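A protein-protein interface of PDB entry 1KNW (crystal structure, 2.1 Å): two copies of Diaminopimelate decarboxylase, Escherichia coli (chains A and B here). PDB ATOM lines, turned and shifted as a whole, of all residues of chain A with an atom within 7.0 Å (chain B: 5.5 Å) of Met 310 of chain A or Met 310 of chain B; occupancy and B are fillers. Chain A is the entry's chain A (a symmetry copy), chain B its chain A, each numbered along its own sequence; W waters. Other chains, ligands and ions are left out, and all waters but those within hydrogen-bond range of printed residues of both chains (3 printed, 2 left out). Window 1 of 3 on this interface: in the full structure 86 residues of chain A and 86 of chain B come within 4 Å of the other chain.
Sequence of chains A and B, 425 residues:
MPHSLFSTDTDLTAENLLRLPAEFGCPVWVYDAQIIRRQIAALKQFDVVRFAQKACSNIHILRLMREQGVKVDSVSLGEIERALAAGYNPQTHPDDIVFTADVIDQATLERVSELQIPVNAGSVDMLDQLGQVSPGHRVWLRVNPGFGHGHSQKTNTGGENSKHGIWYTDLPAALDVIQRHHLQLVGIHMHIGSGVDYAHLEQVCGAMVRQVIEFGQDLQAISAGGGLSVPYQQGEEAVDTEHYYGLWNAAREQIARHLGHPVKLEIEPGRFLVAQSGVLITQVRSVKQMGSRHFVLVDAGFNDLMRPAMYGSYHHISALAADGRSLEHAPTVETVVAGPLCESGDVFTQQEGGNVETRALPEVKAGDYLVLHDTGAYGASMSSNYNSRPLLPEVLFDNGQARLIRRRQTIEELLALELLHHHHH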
ATOM      1  N   PHE A 302      20.411 -12.040  15.555  1.00  0.00           N
ATOM      2  CA  PHE A 302      20.920 -11.252  14.441  1.00  0.00           C
ATOM      3  C   PHE A 302      22.421 -11.040  14.501  1.00  0.00           C
ATOM      4  O   PHE A 302      23.052 -10.838  13.441  1.00  0.00           O
ATOM      5  CB  PHE A 302      20.155 -10.003  14.160  1.00  0.00           C
ATOM      6  CG  PHE A 302      20.383  -8.779  14.987  1.00  0.00           C
ATOM      7  CD1 PHE A 302      21.625  -8.172  15.071  1.00  0.00           C
ATOM      8  CD2 PHE A 302      19.304  -8.127  15.580  1.00  0.00           C
ATOM      9  CE1 PHE A 302      21.814  -7.021  15.813  1.00  0.00           C
ATOM     10  CE2 PHE A 302      19.476  -6.968  16.291  1.00  0.00           C
ATOM     11  CZ  PHE A 302      20.736  -6.406  16.421  1.00  0.00           C
ATOM     12  N   LEU A 305      23.170 -14.211  12.222  1.00  0.00           N
ATOM     13  CA  LEU A 305      22.675 -13.969  10.868  1.00  0.00           C
ATOM     14  C   LEU A 305      22.003 -12.590  10.816  1.00  0.00           C
ATOM     15  O   LEU A 305      20.931 -12.407  11.403  1.00  0.00           O
ATOM     16  CB  LEU A 305      21.638 -15.032  10.472  1.00  0.00           C
ATOM     17  CG  LEU A 305      21.045 -14.841   9.051  1.00  0.00           C
ATOM     18  CD1 LEU A 305      22.096 -15.178   8.009  1.00  0.00           C
ATOM     19  CD2 LEU A 305      19.810 -15.715   8.879  1.00  0.00           C
ATOM     20  N   MET A 306      22.661 -11.625  10.196  1.00  0.00           N
ATOM     21  CA  MET A 306      22.240 -10.242  10.239  1.00  0.00           C
ATOM     22  C   MET A 306      21.083  -9.873   9.310  1.00  0.00           C
ATOM     23  O   MET A 306      20.317  -8.949   9.606  1.00  0.00           O
ATOM     24  CB  MET A 306      23.451  -9.383   9.705  1.00  0.00           C
ATOM     25  CG  MET A 306      24.562  -9.256  10.716  1.00  0.00           C
ATOM     26  SD  MET A 306      24.226  -7.908  11.906  1.00  0.00           S
ATOM     27  CE  MET A 306      25.689  -8.097  12.936  1.00  0.00           C
ATOM     28  N   ARG A 307      21.020 -10.485   8.151  1.00  0.00           N
ATOM     29  CA  ARG A 307      20.118 -10.168   7.086  1.00  0.00           C
ATOM     30  C   ARG A 307      18.703  -9.852   7.374  1.00  0.00           C
ATOM     31  O   ARG A 307      18.207  -8.751   7.000  1.00  0.00           O
ATOM     32  CB  ARG A 307      20.316 -11.127   5.894  1.00  0.00           C
ATOM     33  CG  ARG A 307      21.729 -10.957   5.298  1.00  0.00           C
ATOM     34  CD  ARG A 307      21.928 -11.878   4.098  1.00  0.00           C
ATOM     35  NE  ARG A 307      21.387 -11.300   2.883  1.00  0.00           N
ATOM     36  CZ  ARG A 307      20.294 -11.710   2.262  1.00  0.00           C
ATOM     37  NH1 ARG A 307      19.618 -12.757   2.709  1.00  0.00           N
ATOM     38  NH2 ARG A 307      19.849 -11.080   1.177  1.00  0.00           N
ATOM     39  N   PRO A 308      17.940 -10.736   7.990  1.00  0.00           N
ATOM     40  CA  PRO A 308      16.523 -10.491   8.261  1.00  0.00           C
ATOM     41  C   PRO A 308      16.324  -9.280   9.135  1.00  0.00           C
ATOM     42  O   PRO A 308      15.539  -8.370   8.799  1.00  0.00           O
ATOM     43  CB  PRO A 308      16.047 -11.779   8.903  1.00  0.00           C
ATOM     44  CG  PRO A 308      16.976 -12.825   8.332  1.00  0.00           C
ATOM     45  CD  PRO A 308      18.341 -12.112   8.353  1.00  0.00           C
ATOM     46  N   ALA A 309      17.033  -9.200  10.259  1.00  0.00           N
ATOM     47  CA  ALA A 309      16.862  -8.090  11.185  1.00  0.00           C
ATOM     48  C   ALA A 309      17.312  -6.769  10.595  1.00  0.00           C
ATOM     49  O   ALA A 309      16.650  -5.740  10.789  1.00  0.00           O
ATOM     50  CB  ALA A 309      17.565  -8.347  12.508  1.00  0.00           C
ATOM     51  N   MET A 310      18.473  -6.765   9.936  1.00  0.00           N
ATOM     52  CA  MET A 310      19.008  -5.515   9.413  1.00  0.00           C
ATOM     53  C   MET A 310      18.297  -5.060   8.152  1.00  0.00           C
ATOM     54  O   MET A 310      18.088  -3.851   7.972  1.00  0.00           O
ATOM     55  CB  MET A 310      20.514  -5.623   9.180  1.00  0.00           C
ATOM     56  CG  MET A 310      21.306  -6.050  10.418  1.00  0.00           C
ATOM     57  SD  MET A 310      21.322  -4.820  11.719  1.00  0.00           S
ATOM     58  CE  MET A 310      20.072  -5.414  12.823  1.00  0.00           C
ATOM     59  N   TYR A 311      17.994  -5.971   7.218  1.00  0.00           N
ATOM     60  CA  TYR A 311      17.462  -5.585   5.927  1.00  0.00           C
ATOM     61  C   TYR A 311      16.078  -6.125   5.612  1.00  0.00           C
ATOM     62  O   TYR A 311      15.557  -5.846   4.517  1.00  0.00           O
ATOM     63  CB  TYR A 311      18.417  -6.034   4.800  1.00  0.00           C
ATOM     64  CG  TYR A 311      19.859  -5.655   5.052  1.00  0.00           C
ATOM     65  CD1 TYR A 311      20.804  -6.639   5.341  1.00  0.00           C
ATOM     66  CD2 TYR A 311      20.264  -4.333   5.043  1.00  0.00           C
ATOM     67  CE1 TYR A 311      22.115  -6.304   5.600  1.00  0.00           C
ATOM     68  CE2 TYR A 311      21.580  -3.986   5.300  1.00  0.00           C
ATOM     69  CZ  TYR A 311      22.500  -4.973   5.570  1.00  0.00           C
ATOM     70  OH  TYR A 311      23.809  -4.645   5.810  1.00  0.00           O
ATOM     71  N   GLY A 312      15.548  -7.020   6.428  1.00  0.00           N
ATOM     72  CA  GLY A 312      14.249  -7.635   6.147  1.00  0.00           C
ATOM     73  C   GLY A 312      14.398  -8.765   5.131  1.00  0.00           C
ATOM     74  O   GLY A 312      13.416  -9.146   4.476  1.00  0.00           O
ATOM     75  N   SER A 313      15.606  -9.299   4.994  1.00  0.00           N
ATOM     76  CA  SER A 313      15.878 -10.354   4.039  1.00  0.00           C
ATOM     77  C   SER A 313      15.126 -11.643   4.371  1.00  0.00           C
ATOM     78  O   SER A 313      14.968 -12.036   5.524  1.00  0.00           O
ATOM     79  CB  SER A 313      17.375 -10.666   3.942  1.00  0.00           C
ATOM     80  OG  SER A 313      18.139  -9.528   3.645  1.00  0.00           O
ATOM     81  N   GLU A 343      17.161  -7.432  22.646  1.00  0.00           N
ATOM     82  CA  GLU A 343      17.173  -6.423  21.591  1.00  0.00           C
ATOM     83  C   GLU A 343      15.910  -6.579  20.750  1.00  0.00           C
ATOM     84  O   GLU A 343      15.657  -7.675  20.214  1.00  0.00           O
ATOM     85  CB  GLU A 343      18.427  -6.643  20.732  1.00  0.00           C
ATOM     86  CG  GLU A 343      18.379  -6.026  19.350  1.00  0.00           C
ATOM     87  CD  GLU A 343      18.295  -4.516  19.365  1.00  0.00           C
ATOM     88  OE1 GLU A 343      19.015  -3.884  20.170  1.00  0.00           O
ATOM     89  OE2 GLU A 343      17.498  -3.964  18.580  1.00  0.00           O
ATOM     90  N   GLY A 345      14.898  -5.668  17.804  1.00  0.00           N
ATOM     91  CA  GLY A 345      15.003  -5.969  16.391  1.00  0.00           C
ATOM     92  C   GLY A 345      15.368  -7.400  16.082  1.00  0.00           C
ATOM     93  O   GLY A 345      15.441  -7.761  14.886  1.00  0.00           O
ATOM     94  N   ASP A 346      15.569  -8.250  17.078  1.00  0.00           N
ATOM     95  CA  ASP A 346      16.040  -9.611  16.888  1.00  0.00           C
ATOM     96  C   ASP A 346      14.907 -10.567  16.535  1.00  0.00           C
ATOM     97  O   ASP A 346      14.527 -11.466  17.287  1.00  0.00           O
ATOM     98  CB  ASP A 346      16.796 -10.096  18.126  1.00  0.00           C
ATOM     99  CG  ASP A 346      17.503 -11.419  17.910  1.00  0.00           C
ATOM    100  OD1 ASP A 346      17.665 -12.166  18.893  1.00  0.00           O
ATOM    101  OD2 ASP A 346      17.906 -11.719  16.768  1.00  0.00           O
ATOM    102  N   VAL A 347      14.341 -10.357  15.356  1.00  0.00           N
ATOM    103  CA  VAL A 347      13.222 -11.114  14.823  1.00  0.00           C
ATOM    104  C   VAL A 347      13.543 -11.507  13.366  1.00  0.00           C
ATOM    105  O   VAL A 347      14.021 -10.654  12.599  1.00  0.00           O
ATOM    106  CB  VAL A 347      11.938 -10.260  14.829  1.00  0.00           C
ATOM    107  CG1 VAL A 347      10.808 -10.938  14.070  1.00  0.00           C
ATOM    108  CG2 VAL A 347      11.505  -9.948  16.265  1.00  0.00           C
ATOM    109  N   GLN A 350      10.679 -10.681   9.603  1.00  0.00           N
ATOM    110  CA  GLN A 350      10.306  -9.275   9.516  1.00  0.00           C
ATOM    111  C   GLN A 350      10.591  -8.744   8.114  1.00  0.00           C
ATOM    112  O   GLN A 350      11.489  -9.234   7.420  1.00  0.00           O
ATOM    113  CB  GLN A 350      11.000  -8.437  10.571  1.00  0.00           C
ATOM    114  CG  GLN A 350      12.503  -8.239  10.340  1.00  0.00           C
ATOM    115  CD  GLN A 350      13.071  -7.287  11.389  1.00  0.00           C
ATOM    116  OE1 GLN A 350      12.947  -6.072  11.240  1.00  0.00           O
ATOM    117  NE2 GLN A 350      13.636  -7.845  12.450  1.00  0.00           N
ATOM    118  N   GLU A 352      11.347  -5.624   5.207  1.00  0.00           N
ATOM    119  CA  GLU A 352      12.166  -4.399   5.117  1.00  0.00           C
ATOM    120  C   GLU A 352      11.417  -3.258   5.797  1.00  0.00           C
ATOM    121  O   GLU A 352      10.210  -3.105   5.580  1.00  0.00           O
ATOM    122  CB  GLU A 352      12.412  -4.071   3.647  1.00  0.00           C
ATOM    123  CG  GLU A 352      13.542  -3.078   3.408  1.00  0.00           C
ATOM    124  CD  GLU A 352      13.794  -2.870   1.922  1.00  0.00           C
ATOM    125  OE1 GLU A 352      12.793  -2.773   1.173  1.00  0.00           O
ATOM    126  OE2 GLU A 352      14.965  -2.840   1.511  1.00  0.00           O
ATOM    127  N   GLY A 353      12.092  -2.506   6.651  1.00  0.00           N
ATOM    128  CA  GLY A 353      11.460  -1.418   7.382  1.00  0.00           C
ATOM    129  C   GLY A 353      11.010  -1.827   8.770  1.00  0.00           C
ATOM    130  O   GLY A 353      10.558  -0.988   9.560  1.00  0.00           O
ATOM    131  N   MET A 382      29.176 -11.666   8.142  1.00  0.00           N
ATOM    132  CA  MET A 382      28.704 -10.426   8.757  1.00  0.00           C
ATOM    133  C   MET A 382      28.563 -10.499  10.261  1.00  0.00           C
ATOM    134  O   MET A 382      28.201  -9.473  10.901  1.00  0.00           O
ATOM    135  CB  MET A 382      27.352 -10.027   8.130  1.00  0.00           C
ATOM    136  CG  MET A 382      27.459  -9.657   6.647  1.00  0.00           C
ATOM    137  SD  MET A 382      25.906  -8.927   6.038  1.00  0.00           S
ATOM    138  CE  MET A 382      26.089  -7.242   6.605  1.00  0.00           C
ATOM    139  N   PHE B 302      30.643   0.605   9.014  1.00  0.00           N
ATOM    140  CA  PHE B 302      29.516   0.159   9.820  1.00  0.00           C
ATOM    141  C   PHE B 302      29.837  -1.059  10.666  1.00  0.00           C
ATOM    142  O   PHE B 302      29.197  -1.255  11.721  1.00  0.00           O
ATOM    143  CB  PHE B 302      28.226   0.042   9.079  1.00  0.00           C
ATOM    144  CG  PHE B 302      27.952  -1.156   8.228  1.00  0.00           C
ATOM    145  CD1 PHE B 302      27.934  -2.437   8.753  1.00  0.00           C
ATOM    146  CD2 PHE B 302      27.557  -0.994   6.903  1.00  0.00           C
ATOM    147  CE1 PHE B 302      27.644  -3.533   7.961  1.00  0.00           C
ATOM    148  CE2 PHE B 302      27.239  -2.072   6.118  1.00  0.00           C
ATOM    149  CZ  PHE B 302      27.286  -3.356   6.639  1.00  0.00           C
ATOM    150  N   MET B 306      27.562   0.649  13.959  1.00  0.00           N
ATOM    151  CA  MET B 306      26.485   0.093  13.170  1.00  0.00           C
ATOM    152  C   MET B 306      25.294   1.020  12.931  1.00  0.00           C
ATOM    153  O   MET B 306      24.605   0.899  11.911  1.00  0.00           O
ATOM    154  CB  MET B 306      25.882  -1.102  14.007  1.00  0.00           C
ATOM    155  CG  MET B 306      26.760  -2.327  13.986  1.00  0.00           C
ATOM    156  SD  MET B 306      26.468  -3.327  12.482  1.00  0.00           S
ATOM    157  CE  MET B 306      27.685  -4.618  12.785  1.00  0.00           C
ATOM    158  N   ARG B 307      24.967   1.847  13.896  1.00  0.00           N
ATOM    159  CA  ARG B 307      23.799   2.672  13.932  1.00  0.00           C
ATOM    160  C   ARG B 307      23.351   3.385  12.717  1.00  0.00           C
ATOM    161  O   ARG B 307      22.185   3.201  12.264  1.00  0.00           O
ATOM    162  CB  ARG B 307      23.774   3.536  15.209  1.00  0.00           C
ATOM    163  CG  ARG B 307      23.679   2.639  16.461  1.00  0.00           C
ATOM    164  CD  ARG B 307      23.622   3.481  17.732  1.00  0.00           C
ATOM    165  NE  ARG B 307      22.276   3.945  18.008  1.00  0.00           N
ATOM    166  CZ  ARG B 307      21.855   5.191  17.875  1.00  0.00           C
ATOM    167  NH1 ARG B 307      22.690   6.148  17.509  1.00  0.00           N
ATOM    168  NH2 ARG B 307      20.583   5.508  18.107  1.00  0.00           N
ATOM    169  N   PRO B 308      24.154   4.247  12.121  1.00  0.00           N
ATOM    170  CA  PRO B 308      23.744   5.009  10.941  1.00  0.00           C
ATOM    171  C   PRO B 308      23.386   4.106   9.789  1.00  0.00           C
ATOM    172  O   PRO B 308      22.296   4.230   9.194  1.00  0.00           O
ATOM    173  CB  PRO B 308      24.935   5.903  10.654  1.00  0.00           C
ATOM    174  CG  PRO B 308      25.580   6.080  12.009  1.00  0.00           C
ATOM    175  CD  PRO B 308      25.480   4.668  12.617  1.00  0.00           C
ATOM    176  N   ALA B 309      24.254   3.156   9.450  1.00  0.00           N
ATOM    177  CA  ALA B 309      24.009   2.275   8.317  1.00  0.00           C
ATOM    178  C   ALA B 309      22.821   1.362   8.541  1.00  0.00           C
ATOM    179  O   ALA B 309      22.022   1.139   7.619  1.00  0.00           O
ATOM    180  CB  ALA B 309      25.243   1.464   7.957  1.00  0.00           C
ATOM    181  N   MET B 310      22.731   0.766   9.732  1.00  0.00           N
ATOM    182  CA  MET B 310      21.660  -0.188   9.989  1.00  0.00           C
ATOM    183  C   MET B 310      20.324   0.487  10.232  1.00  0.00           C
ATOM    184  O   MET B 310      19.289  -0.036   9.792  1.00  0.00           O
ATOM    185  CB  MET B 310      22.024  -1.111  11.151  1.00  0.00           C
ATOM    186  CG  MET B 310      23.349  -1.854  10.967  1.00  0.00           C
ATOM    187  SD  MET B 310      23.314  -3.072   9.655  1.00  0.00           S
ATOM    188  CE  MET B 310      24.082  -2.212   8.313  1.00  0.00           C
ATOM    189  N   TYR B 311      20.285   1.586  10.995  1.00  0.00           N
ATOM    190  CA  TYR B 311      19.029   2.186  11.397  1.00  0.00           C
ATOM    191  C   TYR B 311      18.814   3.610  10.916  1.00  0.00           C
ATOM    192  O   TYR B 311      17.763   4.200  11.229  1.00  0.00           O
ATOM    193  CB  TYR B 311      18.902   2.179  12.936  1.00  0.00           C
ATOM    194  CG  TYR B 311      19.210   0.835  13.554  1.00  0.00           C
ATOM    195  CD1 TYR B 311      20.368   0.658  14.311  1.00  0.00           C
ATOM    196  CD2 TYR B 311      18.382  -0.254  13.353  1.00  0.00           C
ATOM    197  CE1 TYR B 311      20.674  -0.570  14.857  1.00  0.00           C
ATOM    198  CE2 TYR B 311      18.680  -1.492  13.899  1.00  0.00           C
ATOM    199  CZ  TYR B 311      19.821  -1.641  14.653  1.00  0.00           C
ATOM    200  OH  TYR B 311      20.119  -2.857  15.213  1.00  0.00           O
ATOM    201  N   GLY B 312      19.819   4.243  10.336  1.00  0.00           N
ATOM    202  CA  GLY B 312      19.702   5.640   9.913  1.00  0.00           C
ATOM    203  C   GLY B 312      19.897   6.580  11.100  1.00  0.00           C
ATOM    204  O   GLY B 312      19.464   7.741  11.052  1.00  0.00           O
HETATM  205  O   HOH W   1      17.496  -2.182  10.145  1.00  0.00           O
HETATM  206  O   HOH W   2      17.762  -3.864  15.785  1.00  0.00           O
HETATM  207  O   HOH W   3      19.323  -1.397   7.342  1.00  0.00           O
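Of chain B, only Met 310 and Tyr 311 come within 4 Å of Met 310 of chain A.
Met 310 of chain B touches two residues of chain A.
Of the printed residues of chain B, Phe 302 of chain A touches Tyr 311 (3.8 Å).
Printed residues of chain A within 4 Å of Phe 302 of chain B: Tyr 311 (3.8 Å).
Of the printed residues of chain A, Tyr 311 of chain B touches Phe 302 (3.8 Å) and Met 310 (3.5 Å).
Of the printed residues of chain B, Tyr 311 of chain A touches Phe 302 (3.8 Å) and Met 310 (3.5 Å).
Pro 308 of chain B touches none of the printed residues of chain A.
Ala 309 of chain B touches none of the printed residues of chain A.
The nearest residue of chain B that does not touch Met 310 of chain A is Met 306 of chain B (5.4 Å).
The nearest residue of chain A that does not touch Met 310 of chain B is Met 306 of chain A (5.4 Å).
Printed residues of chain B that touch a printed residue of chain A: Phe 302, Met 310 and Tyr 311.
Hydrophobic or aromatic side chains of chain B within 4 Å of the printed part of chain A: Phe 302, Met 310 and Tyr 311.
Of the 18 printed residues of chain A, 3 touch a printed residue of chain B.
Printed residues of chain A that touch a printed residue of chain B: Phe 302, Met 310 and Tyr 311.
Hydrophobic or aromatic side chains of chain A within 4 Å of the printed part of chain B: Phe 302, Met 310 and Tyr 311.
Among the printed residues, 5 pairs touch across the chains.
Among the printed residues, no Asp or Glu carboxylate lies within 4 Å of a Lys or Arg side-chain nitrogen of the other chain.
Water W2 lies within hydrogen-bond range of OH of Tyr 311 of chain B (2.6 Å) and OE2 of Glu 343 of chain A (2.8 Å).
Water W1 lies within hydrogen-bond range of the backbone carbonyl oxygen of Met 310 of chain A (2.8 Å) and the backbone carbonyl oxygen of Met 310 of chain B (2.8 Å).
Water W3 lies within hydrogen-bond range of O of Met 310 of chain B and O of Met 310 of chain A.
Among the printed residues, merely in contact across the chains: Phe 302 of chain A with Tyr 311 of chain B (3.8 Å), Met 310 of chain A with Tyr 311 of chain B (3.5 Å), Tyr 311 of chain A with Phe 302 of chain B (3.8 Å) and Tyr 311 of chain A with Met 310 of chain B (3.5 Å).
The side-chain sulfur (SD) of Met 310 of chain A sits close to the side-chain sulfur (SD) of Met 310 of chain B (3.4 Å).
Phe 302 of chain A touches Tyr 311 of chain B, and with the chains exchanged Tyr 311 of chain A touches Phe 302 of chain B.
Met 310 of chain A touches its own counterpart, Met 310 of chain B.
Met 310 of chain A touches Tyr 311 of chain B, and with the chains exchanged Tyr 311 of chain A touches Met 310 of chain B.
8 positions are printed for both chains.
The backbone NH (N) of Phe 302 of chain A is in hydrogen-bond range of the side-chain carboxylate (OD2) of Asp 346 of chain A.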
